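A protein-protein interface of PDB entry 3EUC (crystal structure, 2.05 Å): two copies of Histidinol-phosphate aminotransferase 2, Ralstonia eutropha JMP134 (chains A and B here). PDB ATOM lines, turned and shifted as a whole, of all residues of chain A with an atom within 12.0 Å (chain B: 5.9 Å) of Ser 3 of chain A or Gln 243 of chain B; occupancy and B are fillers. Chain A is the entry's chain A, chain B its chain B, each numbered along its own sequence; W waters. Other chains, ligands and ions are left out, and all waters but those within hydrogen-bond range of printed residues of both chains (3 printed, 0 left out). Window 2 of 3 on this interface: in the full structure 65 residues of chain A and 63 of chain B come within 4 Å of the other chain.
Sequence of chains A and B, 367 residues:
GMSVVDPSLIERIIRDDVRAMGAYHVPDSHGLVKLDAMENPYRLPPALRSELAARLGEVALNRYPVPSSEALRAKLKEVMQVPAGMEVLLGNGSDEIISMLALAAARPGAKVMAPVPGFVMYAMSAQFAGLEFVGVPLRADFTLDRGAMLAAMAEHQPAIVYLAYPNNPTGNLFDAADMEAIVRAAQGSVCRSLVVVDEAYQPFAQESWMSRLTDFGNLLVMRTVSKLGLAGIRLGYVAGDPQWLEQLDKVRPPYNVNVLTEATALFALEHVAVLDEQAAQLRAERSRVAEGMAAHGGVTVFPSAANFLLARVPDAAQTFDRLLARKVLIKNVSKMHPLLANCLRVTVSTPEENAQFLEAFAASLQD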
ATOM      1  N   SER A   3     -26.497  -8.600 -39.984  1.00  0.00           N
ATOM      2  CA  SER A   3     -26.043  -9.746 -39.124  1.00  0.00           C
ATOM      3  C   SER A   3     -26.700 -11.049 -39.616  1.00  0.00           C
ATOM      4  O   SER A   3     -27.917 -11.079 -39.864  1.00  0.00           O
ATOM      5  CB  SER A   3     -26.380  -9.492 -37.644  1.00  0.00           C
ATOM      6  OG  SER A   3     -25.824 -10.501 -36.802  1.00  0.00           O
ATOM      7  N   VAL A   4     -25.885 -12.101 -39.759  1.00  0.00           N
ATOM      8  CA  VAL A   4     -26.329 -13.447 -40.212  1.00  0.00           C
ATOM      9  C   VAL A   4     -26.281 -14.502 -39.044  1.00  0.00           C
ATOM     10  O   VAL A   4     -26.425 -15.704 -39.266  1.00  0.00           O
ATOM     11  CB  VAL A   4     -25.527 -13.856 -41.493  1.00  0.00           C
ATOM     12  CG1 VAL A   4     -24.067 -14.054 -41.190  1.00  0.00           C
ATOM     13  CG2 VAL A   4     -26.123 -15.070 -42.169  1.00  0.00           C
ATOM     14  N   VAL A   5     -26.142 -14.011 -37.805  1.00  0.00           N
ATOM     15  CA  VAL A   5     -26.107 -14.832 -36.594  1.00  0.00           C
ATOM     16  C   VAL A   5     -27.477 -15.460 -36.318  1.00  0.00           C
ATOM     17  O   VAL A   5     -28.515 -14.847 -36.570  1.00  0.00           O
ATOM     18  CB  VAL A   5     -25.639 -14.010 -35.348  1.00  0.00           C
ATOM     19  CG1 VAL A   5     -25.773 -14.792 -34.055  1.00  0.00           C
ATOM     20  CG2 VAL A   5     -24.209 -13.629 -35.497  1.00  0.00           C
ATOM     21  N   ASP A   6     -27.443 -16.700 -35.841  1.00  0.00           N
ATOM     22  CA  ASP A   6     -28.610 -17.466 -35.447  1.00  0.00           C
ATOM     23  C   ASP A   6     -28.580 -17.383 -33.919  1.00  0.00           C
ATOM     24  O   ASP A   6     -27.781 -18.085 -33.303  1.00  0.00           O
ATOM     25  CB  ASP A   6     -28.458 -18.910 -35.954  1.00  0.00           C
ATOM     26  CG  ASP A   6     -29.614 -19.826 -35.555  1.00  0.00           C
ATOM     27  OD1 ASP A   6     -30.504 -19.412 -34.787  1.00  0.00           O
ATOM     28  OD2 ASP A   6     -29.614 -20.985 -36.029  1.00  0.00           O
ATOM     29  N   PRO A   7     -29.431 -16.531 -33.298  1.00  0.00           N
ATOM     30  CA  PRO A   7     -29.395 -16.415 -31.820  1.00  0.00           C
ATOM     31  C   PRO A   7     -29.658 -17.711 -31.048  1.00  0.00           C
ATOM     32  O   PRO A   7     -29.158 -17.849 -29.932  1.00  0.00           O
ATOM     33  CB  PRO A   7     -30.467 -15.351 -31.509  1.00  0.00           C
ATOM     34  CG  PRO A   7     -30.649 -14.620 -32.778  1.00  0.00           C
ATOM     35  CD  PRO A   7     -30.467 -15.641 -33.858  1.00  0.00           C
ATOM     36  N   SER A   8     -30.405 -18.646 -31.637  1.00  0.00           N
ATOM     37  CA  SER A   8     -30.636 -19.947 -31.009  1.00  0.00           C
ATOM     38  C   SER A   8     -29.351 -20.792 -30.957  1.00  0.00           C
ATOM     39  O   SER A   8     -29.231 -21.644 -30.072  1.00  0.00           O
ATOM     40  CB  SER A   8     -31.773 -20.714 -31.678  1.00  0.00           C
ATOM     41  OG  SER A   8     -31.455 -21.104 -32.985  1.00  0.00           O
ATOM     42  N   LEU A   9     -28.413 -20.566 -31.886  1.00  0.00           N
ATOM     43  CA  LEU A   9     -27.111 -21.258 -31.863  1.00  0.00           C
ATOM     44  C   LEU A   9     -26.274 -20.729 -30.692  1.00  0.00           C
ATOM     45  O   LEU A   9     -25.653 -21.505 -29.963  1.00  0.00           O
ATOM     46  CB  LEU A   9     -26.369 -21.125 -33.200  1.00  0.00           C
ATOM     47  CG  LEU A   9     -25.047 -21.884 -33.351  1.00  0.00           C
ATOM     48  CD1 LEU A   9     -25.197 -23.391 -33.065  1.00  0.00           C
ATOM     49  CD2 LEU A   9     -24.474 -21.646 -34.738  1.00  0.00           C
ATOM     50  N   ILE A  10     -26.309 -19.415 -30.482  1.00  0.00           N
ATOM     51  CA  ILE A  10     -25.621 -18.794 -29.348  1.00  0.00           C
ATOM     52  C   ILE A  10     -26.169 -19.363 -28.022  1.00  0.00           C
ATOM     53  O   ILE A  10     -25.397 -19.692 -27.126  1.00  0.00           O
ATOM     54  CB  ILE A  10     -25.705 -17.239 -29.399  1.00  0.00           C
ATOM     55  CG1 ILE A  10     -25.001 -16.734 -30.673  1.00  0.00           C
ATOM     56  CG2 ILE A  10     -25.077 -16.614 -28.121  1.00  0.00           C
ATOM     57  CD1 ILE A  10     -24.809 -15.250 -30.755  1.00  0.00           C
ATOM     58  N   GLU A  11     -27.497 -19.493 -27.941  1.00  0.00           N
ATOM     59  CA  GLU A  11     -28.200 -20.099 -26.789  1.00  0.00           C
ATOM     60  C   GLU A  11     -27.776 -21.548 -26.575  1.00  0.00           C
ATOM     61  O   GLU A  11     -27.573 -21.980 -25.440  1.00  0.00           O
ATOM     62  CB  GLU A  11     -29.726 -20.028 -26.963  1.00  0.00           C
ATOM     63  CG  GLU A  11     -30.281 -18.616 -26.849  1.00  0.00           C
ATOM     64  CD  GLU A  11     -31.705 -18.438 -27.401  1.00  0.00           C
ATOM     65  OE1 GLU A  11     -32.400 -19.437 -27.732  1.00  0.00           O
ATOM     66  OE2 GLU A  11     -32.115 -17.262 -27.518  1.00  0.00           O
ATOM     67  N   ARG A  12     -27.623 -22.277 -27.671  1.00  0.00           N
ATOM     68  CA  ARG A  12     -27.178 -23.663 -27.617  1.00  0.00           C
ATOM     69  C   ARG A  12     -25.693 -23.840 -27.243  1.00  0.00           C
ATOM     70  O   ARG A  12     -25.366 -24.789 -26.532  1.00  0.00           O
ATOM     71  CB  ARG A  12     -27.461 -24.347 -28.955  1.00  0.00           C
ATOM     72  CG  ARG A  12     -27.182 -25.832 -28.961  1.00  0.00           C
ATOM     73  CD  ARG A  12     -27.665 -26.467 -30.225  1.00  0.00           C
ATOM     74  NE  ARG A  12     -27.525 -27.919 -30.136  1.00  0.00           N
ATOM     75  CZ  ARG A  12     -28.355 -28.742 -29.484  1.00  0.00           C
ATOM     76  NH1 ARG A  12     -29.470 -28.307 -28.874  1.00  0.00           N
ATOM     77  NH2 ARG A  12     -28.076 -30.047 -29.479  1.00  0.00           N
ATOM     78  N   ILE A  13     -24.815 -22.947 -27.714  1.00  0.00           N
ATOM     79  CA  ILE A  13     -23.346 -23.078 -27.523  1.00  0.00           C
ATOM     80  C   ILE A  13     -22.808 -22.483 -26.227  1.00  0.00           C
ATOM     81  O   ILE A  13     -21.997 -23.104 -25.582  1.00  0.00           O
ATOM     82  CB  ILE A  13     -22.546 -22.483 -28.748  1.00  0.00           C
ATOM     83  CG1 ILE A  13     -22.868 -23.234 -30.048  1.00  0.00           C
ATOM     84  CG2 ILE A  13     -21.033 -22.516 -28.510  1.00  0.00           C
ATOM     85  CD1 ILE A  13     -22.471 -24.696 -30.057  1.00  0.00           C
ATOM     86  N   ILE A  14     -23.254 -21.287 -25.867  1.00  0.00           N
ATOM     87  CA  ILE A  14     -22.788 -20.604 -24.659  1.00  0.00           C
ATOM     88  C   ILE A  14     -23.550 -21.133 -23.421  1.00  0.00           C
ATOM     89  O   ILE A  14     -24.757 -21.396 -23.495  1.00  0.00           O
ATOM     90  CB  ILE A  14     -22.962 -19.051 -24.777  1.00  0.00           C
ATOM     91  CG1 ILE A  14     -22.256 -18.497 -26.031  1.00  0.00           C
ATOM     92  CG2 ILE A  14     -22.418 -18.338 -23.506  1.00  0.00           C
ATOM     93  CD1 ILE A  14     -20.734 -18.724 -26.065  1.00  0.00           C
ATOM     94  N   ARG A  15     -22.827 -21.317 -22.307  1.00  0.00           N
ATOM     95  CA  ARG A  15     -23.414 -21.738 -21.015  1.00  0.00           C
ATOM     96  C   ARG A  15     -24.536 -20.798 -20.582  1.00  0.00           C
ATOM     97  O   ARG A  15     -24.407 -19.592 -20.769  1.00  0.00           O
ATOM     98  CB  ARG A  15     -22.354 -21.760 -19.898  1.00  0.00           C
ATOM     99  CG  ARG A  15     -21.333 -22.898 -19.943  1.00  0.00           C
ATOM    100  CD  ARG A  15     -20.330 -22.887 -18.741  1.00  0.00           C
ATOM    101  NE  ARG A  15     -20.957 -22.962 -17.397  1.00  0.00           N
ATOM    102  CZ  ARG A  15     -21.394 -24.073 -16.758  1.00  0.00           C
ATOM    103  NH1 ARG A  15     -21.325 -25.292 -17.293  1.00  0.00           N
ATOM    104  NH2 ARG A  15     -21.962 -23.963 -15.553  1.00  0.00           N
ATOM    105  N   VAL A  18     -23.372 -18.159 -18.234  1.00  0.00           N
ATOM    106  CA  VAL A  18     -22.597 -17.107 -18.913  1.00  0.00           C
ATOM    107  C   VAL A  18     -23.572 -16.130 -19.575  1.00  0.00           C
ATOM    108  O   VAL A  18     -23.417 -14.925 -19.405  1.00  0.00           O
ATOM    109  CB  VAL A  18     -21.544 -17.690 -19.890  1.00  0.00           C
ATOM    110  CG1 VAL A  18     -20.887 -16.594 -20.732  1.00  0.00           C
ATOM    111  CG2 VAL A  18     -20.497 -18.454 -19.095  1.00  0.00           C
ATOM    112  N   ARG A  19     -24.580 -16.642 -20.292  1.00  0.00           N
ATOM    113  CA  ARG A  19     -25.611 -15.781 -20.901  1.00  0.00           C
ATOM    114  C   ARG A  19     -26.476 -15.054 -19.868  1.00  0.00           C
ATOM    115  O   ARG A  19     -26.948 -13.954 -20.153  1.00  0.00           O
ATOM    116  CB  ARG A  19     -26.539 -16.553 -21.834  1.00  0.00           C
ATOM    117  CG  ARG A  19     -25.863 -17.231 -23.013  1.00  0.00           C
ATOM    118  CD  ARG A  19     -26.859 -17.500 -24.137  1.00  0.00           C
ATOM    119  NE  ARG A  19     -28.133 -18.034 -23.642  1.00  0.00           N
ATOM    120  CZ  ARG A  19     -28.352 -19.286 -23.229  1.00  0.00           C
ATOM    121  NH1 ARG A  19     -27.381 -20.189 -23.233  1.00  0.00           N
ATOM    122  NH2 ARG A  19     -29.566 -19.633 -22.808  1.00  0.00           N
ATOM    123  N   ALA A  20     -26.712 -15.699 -18.713  1.00  0.00           N
ATOM    124  CA  ALA A  20     -27.454 -15.113 -17.578  1.00  0.00           C
ATOM    125  C   ALA A  20     -26.778 -13.847 -17.058  1.00  0.00           C
ATOM    126  O   ALA A  20     -27.463 -12.858 -16.779  1.00  0.00           O
ATOM    127  CB  ALA A  20     -27.597 -16.116 -16.433  1.00  0.00           C
ATOM    128  N   MET A  21     -25.445 -13.878 -16.950  1.00  0.00           N
ATOM    129  CA  MET A  21     -24.658 -12.715 -16.503  1.00  0.00           C
ATOM    130  C   MET A  21     -24.838 -11.537 -17.450  1.00  0.00           C
ATOM    131  O   MET A  21     -24.968 -11.720 -18.669  1.00  0.00           O
ATOM    132  CB  MET A  21     -23.154 -13.011 -16.455  1.00  0.00           C
ATOM    133  CG  MET A  21     -22.713 -14.057 -15.470  1.00  0.00           C
ATOM    134  SD  MET A  21     -20.902 -14.630 -15.959  1.00  0.00           S
ATOM    135  CE  MET A  21     -21.052 -16.429 -15.593  1.00  0.00           C
ATOM    136  N   GLY A  22     -24.846 -10.338 -16.869  1.00  0.00           N
ATOM    137  CA  GLY A  22     -24.920  -9.091 -17.622  1.00  0.00           C
ATOM    138  C   GLY A  22     -23.509  -8.687 -18.012  1.00  0.00           C
ATOM    139  O   GLY A  22     -22.552  -9.455 -17.808  1.00  0.00           O
ATOM    140  N   ALA A  23     -23.387  -7.473 -18.553  1.00  0.00           N
ATOM    141  CA  ALA A  23     -22.101  -6.904 -18.993  1.00  0.00           C
ATOM    142  C   ALA A  23     -20.994  -6.990 -17.914  1.00  0.00           C
ATOM    143  O   ALA A  23     -20.962  -6.183 -16.969  1.00  0.00           O
ATOM    144  CB  ALA A  23     -22.287  -5.431 -19.465  1.00  0.00           C
ATOM    145  N   MET B  86     -18.588  -6.210 -37.342  1.00  0.00           N
ATOM    146  CA  MET B  86     -17.852  -7.231 -36.558  1.00  0.00           C
ATOM    147  C   MET B  86     -16.970  -6.515 -35.553  1.00  0.00           C
ATOM    148  O   MET B  86     -16.544  -5.392 -35.816  1.00  0.00           O
ATOM    149  CB  MET B  86     -16.987  -8.095 -37.474  1.00  0.00           C
ATOM    150  CG  MET B  86     -17.724  -8.717 -38.641  1.00  0.00           C
ATOM    151  SD  MET B  86     -19.113  -9.859 -38.029  1.00  0.00           S
ATOM    152  CE  MET B  86     -20.416  -9.559 -39.439  1.00  0.00           C
ATOM    153  N   ASP B 241     -18.928 -11.577 -34.830  1.00  0.00           N
ATOM    154  CA  ASP B 241     -20.140 -10.820 -34.549  1.00  0.00           C
ATOM    155  C   ASP B 241     -20.235 -10.470 -33.057  1.00  0.00           C
ATOM    156  O   ASP B 241     -19.973 -11.339 -32.229  1.00  0.00           O
ATOM    157  CB  ASP B 241     -21.375 -11.648 -34.941  1.00  0.00           C
ATOM    158  CG  ASP B 241     -22.649 -10.832 -34.970  1.00  0.00           C
ATOM    159  OD1 ASP B 241     -23.262 -10.623 -33.911  1.00  0.00           O
ATOM    160  OD2 ASP B 241     -23.078 -10.464 -36.080  1.00  0.00           O
ATOM    161  N   PRO B 242     -20.625  -9.221 -32.706  1.00  0.00           N
ATOM    162  CA  PRO B 242     -20.846  -8.820 -31.307  1.00  0.00           C
ATOM    163  C   PRO B 242     -21.659  -9.800 -30.456  1.00  0.00           C
ATOM    164  O   PRO B 242     -21.377  -9.929 -29.275  1.00  0.00           O
ATOM    165  CB  PRO B 242     -21.625  -7.506 -31.435  1.00  0.00           C
ATOM    166  CG  PRO B 242     -21.272  -6.966 -32.750  1.00  0.00           C
ATOM    167  CD  PRO B 242     -20.805  -8.076 -33.620  1.00  0.00           C
ATOM    168  N   GLN B 243     -22.651 -10.475 -31.047  1.00  0.00           N
ATOM    169  CA  GLN B 243     -23.477 -11.431 -30.307  1.00  0.00           C
ATOM    170  C   GLN B 243     -22.661 -12.617 -29.808  1.00  0.00           C
ATOM    171  O   GLN B 243     -22.991 -13.192 -28.771  1.00  0.00           O
ATOM    172  CB  GLN B 243     -24.689 -11.873 -31.116  1.00  0.00           C
ATOM    173  CG  GLN B 243     -25.636 -10.738 -31.422  1.00  0.00           C
ATOM    174  CD  GLN B 243     -26.814 -11.163 -32.281  1.00  0.00           C
ATOM    175  OE1 GLN B 243     -27.608 -12.024 -31.885  1.00  0.00           O
ATOM    176  NE2 GLN B 243     -26.944 -10.545 -33.459  1.00  0.00           N
ATOM    177  N   TRP B 244     -21.611 -12.993 -30.544  1.00  0.00           N
ATOM    178  CA  TRP B 244     -20.666 -13.976 -30.054  1.00  0.00           C
ATOM    179  C   TRP B 244     -19.719 -13.332 -29.047  1.00  0.00           C
ATOM    180  O   TRP B 244     -19.595 -13.825 -27.927  1.00  0.00           O
ATOM    181  CB  TRP B 244     -19.826 -14.595 -31.168  1.00  0.00           C
ATOM    182  CG  TRP B 244     -20.548 -15.591 -31.977  1.00  0.00           C
ATOM    183  CD1 TRP B 244     -20.836 -15.507 -33.303  1.00  0.00           C
ATOM    184  CD2 TRP B 244     -21.078 -16.848 -31.526  1.00  0.00           C
ATOM    185  NE1 TRP B 244     -21.502 -16.632 -33.707  1.00  0.00           N
ATOM    186  CE2 TRP B 244     -21.675 -17.469 -32.640  1.00  0.00           C
ATOM    187  CE3 TRP B 244     -21.103 -17.512 -30.288  1.00  0.00           C
ATOM    188  CZ2 TRP B 244     -22.300 -18.723 -32.558  1.00  0.00           C
ATOM    189  CZ3 TRP B 244     -21.743 -18.750 -30.202  1.00  0.00           C
ATOM    190  CH2 TRP B 244     -22.316 -19.346 -31.331  1.00  0.00           C
ATOM    191  N   LEU B 245     -19.068 -12.237 -29.444  1.00  0.00           N
ATOM    192  CA  LEU B 245     -18.015 -11.652 -28.618  1.00  0.00           C
ATOM    193  C   LEU B 245     -18.479 -11.055 -27.300  1.00  0.00           C
ATOM    194  O   LEU B 245     -17.684 -11.039 -26.362  1.00  0.00           O
ATOM    195  CB  LEU B 245     -17.109 -10.676 -29.388  1.00  0.00           C
ATOM    196  CG  LEU B 245     -16.420 -11.133 -30.683  1.00  0.00           C
ATOM    197  CD1 LEU B 245     -15.331 -10.121 -31.057  1.00  0.00           C
ATOM    198  CD2 LEU B 245     -15.836 -12.522 -30.610  1.00  0.00           C
ATOM    199  N   GLU B 246     -19.729 -10.580 -27.225  1.00  0.00           N
ATOM    200  CA  GLU B 246     -20.307 -10.059 -25.972  1.00  0.00           C
ATOM    201  C   GLU B 246     -20.426 -11.155 -24.916  1.00  0.00           C
ATOM    202  O   GLU B 246     -20.433 -10.867 -23.720  1.00  0.00           O
ATOM    203  CB  GLU B 246     -21.695  -9.404 -26.171  1.00  0.00           C
ATOM    204  CG  GLU B 246     -22.888 -10.371 -26.461  1.00  0.00           C
ATOM    205  CD  GLU B 246     -24.239  -9.672 -26.558  1.00  0.00           C
ATOM    206  OE1 GLU B 246     -24.508  -8.743 -25.777  1.00  0.00           O
ATOM    207  OE2 GLU B 246     -25.060 -10.095 -27.383  1.00  0.00           O
ATOM    208  N   GLN B 247     -20.561 -12.409 -25.366  1.00  0.00           N
ATOM    209  CA  GLN B 247     -20.682 -13.557 -24.478  1.00  0.00           C
ATOM    210  C   GLN B 247     -19.282 -14.019 -24.078  1.00  0.00           C
ATOM    211  O   GLN B 247     -19.031 -14.276 -22.905  1.00  0.00           O
ATOM    212  CB  GLN B 247     -21.461 -14.692 -25.153  1.00  0.00           C
ATOM    213  CG  GLN B 247     -22.878 -14.314 -25.576  1.00  0.00           C
ATOM    214  CD  GLN B 247     -23.801 -13.995 -24.414  1.00  0.00           C
ATOM    215  OE1 GLN B 247     -23.533 -14.347 -23.268  1.00  0.00           O
ATOM    216  NE2 GLN B 247     -24.902 -13.328 -24.715  1.00  0.00           N
HETATM  217  O   HOH W   1     -25.019  -8.682 -34.113  1.00  0.00           O
HETATM  218  O   HOH W   2     -26.883 -12.722 -22.841  1.00  0.00           O
HETATM  219  O   HOH W   3     -22.856 -11.958 -38.519  1.00  0.00           O
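OG of Ser 3 of chain A sits at hydrogen-bond distance from OD2 of Asp 241 of chain B, at 2.8 Å.
The guanidinium group (NH1) of Arg 19 of chain A is in hydrogen-bond range of the backbone carbonyl oxygen (O) of Glu 11 of chain A, at 2.8 Å. O of Ile 14 of chain A sits at hydrogen-bond distance from NH1 of Arg 19 of chain A (2.9 Å). The side-chain sulfur (SD) of Met 86 of chain B is in hydrogen-bond range of the backbone NH (N) of Asp 241 of chain B (3.6 Å). N of Gln 243 of chain B is in hydrogen-bond range of OD1 of Asp 241 of chain B (2.9 Å).
No position is printed for both chains. Of the 9 pairs that touch across the chains among the printed residues, none has its exchanged pair printed and touching as well.
Of chain B, only Asp 241 and Gln 243 come within 4 Å of Ser 3 of chain A. Of the printed residues of chain B, Ile 10 of chain A touches Gln 243 (3.4 Å) and Trp 244 (3.8 Å). Of the printed residues of chain B, Ile 14 of chain A touches Gln 247. Arg 15 of chain A touches none of the printed residues of chain B. Printed residues of chain B within 4 Å of Val 18 of chain A: Gln 247. Of the printed residues of chain B, Arg 19 of chain A touches Gln 247. Met 21 of chain A touches none of the printed residues of chain B. Of the printed residues of chain A, Gln 247 of chain B touches Ile 14, Val 18 and Arg 19. The nearest residue of chain B that does not touch Ser 3 of chain A is Met 86 of chain B (5.6 Å). The nearest printed residue of chain B that does not touch Val 18 of chain A is Glu 246 of chain B (6.5 Å).
Of the 19 printed residues of chain A, 6 touch a printed residue of chain B. Hydrophobic or aromatic side chains of chain A that line the printed part of chain B: Val 5, Ile 10, Ile 14 and Val 18. Of the 8 printed residues of chain B, 4 touch a printed residue of chain A. Among the printed residues, 9 pairs touch across the chains. Among the printed residues, no Asp or Glu carboxylate lies within 4 Å of a Lys or Arg side-chain nitrogen of the other chain.
Among the printed residues, merely in contact across the chains: Ser 3 of chain A with Gln 243 of chain B (3.5 Å), Val 5 of chain A with Asp 241 of chain B (3.2 Å), Val 5 of chain A with Gln 243 of chain B (3.97 Å), Ile 10 of chain A with Gln 243 of chain B (3.4 Å), Ile 10 of chain A with Trp 244 of chain B (3.8 Å), Ile 14 of chain A with Gln 247 of chain B (3.99 Å), Val 18 of chain A with Gln 247 of chain B (3.7 Å) and Arg 19 of chain A with Gln 247 of chain B (3.5 Å).
Water W1 lies within hydrogen-bond range of OD1 of Asp 241 of chain B (2.6 Å), NE2 of Gln 243 of chain B (2.8 Å) and OG of Ser 3 of chain A (3.3 Å). Water W2 bridges NE2 of Gln 247 of chain B (2.8 Å) and O of Arg 19 of chain A (3.0 Å). Water W3 bridges OD2 of Asp 241 of chain B (2.9 Å) and N of Val 4 of chain A (3.3 Å).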
